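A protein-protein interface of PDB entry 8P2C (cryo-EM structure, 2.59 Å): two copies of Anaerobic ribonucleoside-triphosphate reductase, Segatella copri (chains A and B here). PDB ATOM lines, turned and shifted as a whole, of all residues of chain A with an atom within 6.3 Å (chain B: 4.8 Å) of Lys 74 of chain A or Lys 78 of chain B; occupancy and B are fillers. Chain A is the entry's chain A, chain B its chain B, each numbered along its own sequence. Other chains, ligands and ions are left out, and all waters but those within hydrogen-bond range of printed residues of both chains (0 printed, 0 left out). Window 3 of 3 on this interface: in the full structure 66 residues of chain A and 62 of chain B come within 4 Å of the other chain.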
ATOM      1  N   GLU A  69       2.962  10.040 -23.178  1.00  0.00           N
ATOM      2  CA  GLU A  69       3.940   9.009 -23.507  1.00  0.00           C
ATOM      3  C   GLU A  69       4.894   8.759 -22.347  1.00  0.00           C
ATOM      4  O   GLU A  69       5.192   7.607 -22.012  1.00  0.00           O
ATOM      5  CB  GLU A  69       4.719   9.399 -24.761  1.00  0.00           C
ATOM      6  CG  GLU A  69       4.031   9.041 -26.058  1.00  0.00           C
ATOM      7  CD  GLU A  69       4.898   9.324 -27.263  1.00  0.00           C
ATOM      8  OE1 GLU A  69       5.990   9.902 -27.084  1.00  0.00           O
ATOM      9  OE2 GLU A  69       4.491   8.968 -28.388  1.00  0.00           O
ATOM     10  N   MET A  70       5.378   9.823 -21.717  1.00  0.00           N
ATOM     11  CA  MET A  70       6.371   9.677 -20.656  1.00  0.00           C
ATOM     12  C   MET A  70       5.699   9.541 -19.295  1.00  0.00           C
ATOM     13  O   MET A  70       6.345   9.463 -18.252  1.00  0.00           O
ATOM     14  CB  MET A  70       7.332  10.857 -20.688  1.00  0.00           C
ATOM     15  CG  MET A  70       8.614  10.656 -19.903  1.00  0.00           C
ATOM     16  SD  MET A  70       9.890  11.830 -20.385  1.00  0.00           S
ATOM     17  CE  MET A  70      10.160  11.344 -22.088  1.00  0.00           C
ATOM     18  N   GLU A  71       4.370   9.471 -19.310  1.00  0.00           N
ATOM     19  CA  GLU A  71       3.635   9.149 -18.095  1.00  0.00           C
ATOM     20  C   GLU A  71       2.994   7.773 -18.139  1.00  0.00           C
ATOM     21  O   GLU A  71       2.545   7.294 -17.095  1.00  0.00           O
ATOM     22  CB  GLU A  71       2.551  10.206 -17.832  1.00  0.00           C
ATOM     23  CG  GLU A  71       2.175  10.381 -16.367  1.00  0.00           C
ATOM     24  CD  GLU A  71       3.266  11.060 -15.563  1.00  0.00           C
ATOM     25  OE1 GLU A  71       4.098  11.764 -16.171  1.00  0.00           O
ATOM     26  OE2 GLU A  71       3.297  10.892 -14.324  1.00  0.00           O
ATOM     27  N   LEU A  72       2.938   7.121 -19.297  1.00  0.00           N
ATOM     28  CA  LEU A  72       2.631   5.701 -19.378  1.00  0.00           C
ATOM     29  C   LEU A  72       3.878   4.832 -19.302  1.00  0.00           C
ATOM     30  O   LEU A  72       3.758   3.620 -19.105  1.00  0.00           O
ATOM     31  CB  LEU A  72       1.881   5.392 -20.678  1.00  0.00           C
ATOM     32  CG  LEU A  72       0.429   5.848 -20.779  1.00  0.00           C
ATOM     33  CD1 LEU A  72      -0.023   5.831 -22.226  1.00  0.00           C
ATOM     34  CD2 LEU A  72      -0.451   4.953 -19.934  1.00  0.00           C
ATOM     35  N   MET A  73       5.061   5.421 -19.459  1.00  0.00           N
ATOM     36  CA  MET A  73       6.324   4.716 -19.309  1.00  0.00           C
ATOM     37  C   MET A  73       6.834   4.736 -17.876  1.00  0.00           C
ATOM     38  O   MET A  73       7.891   4.160 -17.598  1.00  0.00           O
ATOM     39  CB  MET A  73       7.376   5.314 -20.242  1.00  0.00           C
ATOM     40  CG  MET A  73       7.205   4.942 -21.699  1.00  0.00           C
ATOM     41  SD  MET A  73       8.449   5.718 -22.740  1.00  0.00           S
ATOM     42  CE  MET A  73       8.670   4.465 -23.996  1.00  0.00           C
ATOM     43  N   LYS A  74       6.115   5.392 -16.968  1.00  0.00           N
ATOM     44  CA  LYS A  74       6.439   5.381 -15.552  1.00  0.00           C
ATOM     45  C   LYS A  74       5.350   4.732 -14.715  1.00  0.00           C
ATOM     46  O   LYS A  74       5.477   4.689 -13.485  1.00  0.00           O
ATOM     47  CB  LYS A  74       6.683   6.808 -15.043  1.00  0.00           C
ATOM     48  CG  LYS A  74       7.770   7.560 -15.785  1.00  0.00           C
ATOM     49  CD  LYS A  74       7.933   8.969 -15.242  1.00  0.00           C
ATOM     50  CE  LYS A  74       9.031   9.719 -15.978  1.00  0.00           C
ATOM     51  NZ  LYS A  74       9.206  11.101 -15.457  1.00  0.00           N
ATOM     52  N   SER A  75       4.291   4.230 -15.337  1.00  0.00           N
ATOM     53  CA  SER A  75       3.187   3.615 -14.622  1.00  0.00           C
ATOM     54  C   SER A  75       3.435   2.115 -14.490  1.00  0.00           C
ATOM     55  O   SER A  75       4.491   1.600 -14.866  1.00  0.00           O
ATOM     56  CB  SER A  75       1.869   3.911 -15.332  1.00  0.00           C
ATOM     57  OG  SER A  75       1.862   3.360 -16.637  1.00  0.00           O
ATOM     58  N   ALA A  76       2.454   1.396 -13.954  1.00  0.00           N
ATOM     59  CA  ALA A  76       2.562  -0.039 -13.749  1.00  0.00           C
ATOM     60  C   ALA A  76       1.976  -0.842 -14.897  1.00  0.00           C
ATOM     61  O   ALA A  76       1.960  -2.075 -14.828  1.00  0.00           O
ATOM     62  CB  ALA A  76       1.880  -0.439 -12.438  1.00  0.00           C
ATOM     63  N   LYS A  78       2.860  -0.953 -18.644  1.00  0.00           N
ATOM     64  CA  LYS A  78       3.678  -0.588 -19.788  1.00  0.00           C
ATOM     65  C   LYS A  78       3.272  -1.319 -21.059  1.00  0.00           C
ATOM     66  O   LYS A  78       3.831  -1.035 -22.124  1.00  0.00           O
ATOM     67  CB  LYS A  78       5.153  -0.853 -19.483  1.00  0.00           C
ATOM     68  CG  LYS A  78       5.676  -0.086 -18.283  1.00  0.00           C
ATOM     69  CD  LYS A  78       7.120  -0.438 -17.987  1.00  0.00           C
ATOM     70  CE  LYS A  78       7.655   0.371 -16.820  1.00  0.00           C
ATOM     71  NZ  LYS A  78       6.885   0.123 -15.576  1.00  0.00           N
ATOM     72  N   LEU B  72      14.538  -0.623 -21.320  1.00  0.00           N
ATOM     73  CA  LEU B  72      14.745   0.776 -21.666  1.00  0.00           C
ATOM     74  C   LEU B  72      13.642   1.686 -21.138  1.00  0.00           C
ATOM     75  O   LEU B  72      13.858   2.899 -21.044  1.00  0.00           O
ATOM     76  CB  LEU B  72      14.857   0.937 -23.183  1.00  0.00           C
ATOM     77  CG  LEU B  72      16.129   0.415 -23.843  1.00  0.00           C
ATOM     78  CD1 LEU B  72      16.139   0.751 -25.320  1.00  0.00           C
ATOM     79  CD2 LEU B  72      17.356   0.981 -23.158  1.00  0.00           C
ATOM     80  N   MET B  73      12.479   1.139 -20.795  1.00  0.00           N
ATOM     81  CA  MET B  73      11.410   1.923 -20.191  1.00  0.00           C
ATOM     82  C   MET B  73      11.591   2.113 -18.692  1.00  0.00           C
ATOM     83  O   MET B  73      10.757   2.768 -18.060  1.00  0.00           O
ATOM     84  CB  MET B  73      10.050   1.272 -20.463  1.00  0.00           C
ATOM     85  CG  MET B  73       9.557   1.428 -21.887  1.00  0.00           C
ATOM     86  SD  MET B  73       7.898   0.774 -22.134  1.00  0.00           S
ATOM     87  CE  MET B  73       8.143  -0.948 -21.716  1.00  0.00           C
ATOM     88  N   ALA B  76      15.636   5.480 -16.888  1.00  0.00           N
ATOM     89  CA  ALA B  76      15.784   6.936 -16.839  1.00  0.00           C
ATOM     90  C   ALA B  76      16.334   7.482 -18.154  1.00  0.00           C
ATOM     91  O   ALA B  76      16.984   8.527 -18.188  1.00  0.00           O
ATOM     92  CB  ALA B  76      16.663   7.376 -15.663  1.00  0.00           C
ATOM     93  N   ARG B  77      16.079   6.759 -19.239  1.00  0.00           N
ATOM     94  CA  ARG B  77      16.545   7.104 -20.574  1.00  0.00           C
ATOM     95  C   ARG B  77      15.425   6.837 -21.572  1.00  0.00           C
ATOM     96  O   ARG B  77      15.614   6.203 -22.611  1.00  0.00           O
ATOM     97  CB  ARG B  77      17.808   6.323 -20.922  1.00  0.00           C
ATOM     98  CG  ARG B  77      18.575   6.871 -22.099  1.00  0.00           C
ATOM     99  CD  ARG B  77      19.189   8.208 -21.778  1.00  0.00           C
ATOM    100  NE  ARG B  77      20.595   8.233 -22.155  1.00  0.00           N
ATOM    101  CZ  ARG B  77      21.039   8.549 -23.361  1.00  0.00           C
ATOM    102  NH1 ARG B  77      20.212   8.900 -24.332  1.00  0.00           N
ATOM    103  NH2 ARG B  77      22.346   8.518 -23.600  1.00  0.00           N
ATOM    104  N   LYS B  78      14.230   7.319 -21.250  1.00  0.00           N
ATOM    105  CA  LYS B  78      13.021   6.973 -21.983  1.00  0.00           C
ATOM    106  C   LYS B  78      12.934   7.638 -23.349  1.00  0.00           C
ATOM    107  O   LYS B  78      11.868   7.603 -23.970  1.00  0.00           O
ATOM    108  CB  LYS B  78      11.796   7.329 -21.141  1.00  0.00           C
ATOM    109  CG  LYS B  78      11.836   6.711 -19.759  1.00  0.00           C
ATOM    110  CD  LYS B  78      10.655   7.132 -18.915  1.00  0.00           C
ATOM    111  CE  LYS B  78      10.663   6.406 -17.584  1.00  0.00           C
ATOM    112  NZ  LYS B  78      11.926   6.639 -16.834  1.00  0.00           N
ATOM    113  N   ASP B  79      14.019   8.244 -23.829  1.00  0.00           N
ATOM    114  CA  ASP B  79      14.065   8.782 -25.179  1.00  0.00           C
ATOM    115  C   ASP B  79      14.627   7.798 -26.191  1.00  0.00           C
ATOM    116  O   ASP B  79      14.400   7.971 -27.393  1.00  0.00           O
ATOM    117  CB  ASP B  79      14.905  10.063 -25.209  1.00  0.00           C
ATOM    118  CG  ASP B  79      16.311   9.847 -24.692  1.00  0.00           C
ATOM    119  OD1 ASP B  79      16.497   8.968 -23.825  1.00  0.00           O
ATOM    120  OD2 ASP B  79      17.231  10.555 -25.152  1.00  0.00           O
ATOM    121  N   VAL B  80      15.356   6.781 -25.736  1.00  0.00           N
ATOM    122  CA  VAL B  80      15.825   5.726 -26.623  1.00  0.00           C
ATOM    123  C   VAL B  80      14.739   4.682 -26.864  1.00  0.00           C
ATOM    124  O   VAL B  80      14.651   4.119 -27.963  1.00  0.00           O
ATOM    125  CB  VAL B  80      17.096   5.081 -26.045  1.00  0.00           C
ATOM    126  CG1 VAL B  80      17.719   4.128 -27.050  1.00  0.00           C
ATOM    127  CG2 VAL B  80      18.084   6.152 -25.636  1.00  0.00           C
ATOM    128  N   ALA B  81      13.899   4.427 -25.861  1.00  0.00           N
ATOM    129  CA  ALA B  81      12.813   3.471 -26.019  1.00  0.00           C
ATOM    130  C   ALA B  81      11.822   3.915 -27.084  1.00  0.00           C
ATOM    131  O   ALA B  81      11.305   3.080 -27.832  1.00  0.00           O
ATOM    132  CB  ALA B  81      12.101   3.267 -24.684  1.00  0.00           C
ATOM    133  N   GLN B  82      11.538   5.217 -27.168  1.00  0.00           N
ATOM    134  CA  GLN B  82      10.566   5.696 -28.142  1.00  0.00           C
ATOM    135  C   GLN B  82      11.074   5.587 -29.573  1.00  0.00           C
ATOM    136  O   GLN B  82      10.264   5.440 -30.493  1.00  0.00           O
ATOM    137  CB  GLN B  82      10.178   7.138 -27.827  1.00  0.00           C
ATOM    138  CG  GLN B  82       9.474   7.301 -26.494  1.00  0.00           C
ATOM    139  CD  GLN B  82       9.061   8.730 -26.224  1.00  0.00           C
ATOM    140  OE1 GLN B  82       9.241   9.610 -27.067  1.00  0.00           O
ATOM    141  NE2 GLN B  82       8.503   8.973 -25.045  1.00  0.00           N
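Hydrophobic or aromatic side chains of chain A that line the printed part of chain B: Met 73. Among the printed residues, no Asp or Glu carboxylate lies within 4 Å of a Lys or Arg side-chain nitrogen of the other chain.
Met 73 of chain A touches its own counterpart, Met 73 of chain B. Met 73 of chain A touches Lys 78 of chain B, and with the chains exchanged Lys 78 of chain A touches Met 73 of chain B. 4 positions are printed for both chains. Of the 7 pairs that touch across the chains among the printed residues, 3 have their exchanged pair printed and touching as well.
NZ of Lys 78 of chain A sits at hydrogen-bond distance from O of Ser 75 of chain A.
Among the printed residues, pairs that only touch across the chains: Met 73 of chain A with Lys 78 of chain B, Lys 74 of chain A with Lys 78 of chain B, Met 73 of chain A with Ala 81 of chain B, Lys 78 of chain A with Met 73 of chain B and Met 73 of chain A with Gln 82 of chain B.
Of chain B, only Lys 78 (3.6 Å) comes within 4 Å of Lys 74 of chain A. Of the printed residues of chain B, Lys 78 of chain A touches Met 73 (3.7 Å). Of chain A, only Met 73 (3.6 Å) and Lys 74 (3.6 Å) come within 4 Å of Lys 78 of chain B. Of the printed residues of chain A, Ala 81 of chain B touches Met 73 (3.7 Å). The nearest printed residue of chain B that does not touch Lys 78 of chain A is Lys 78 of chain B (6.8 Å).
The backbone carbonyl oxygen (O) of Met 73 of chain A lies close to the backbone carbonyl oxygen (O) of Met 73 of chain B (3.2 Å). OE1 of Glu 69 of chain A sits close to OE1 of Gln 82 of chain B (3.3 Å).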
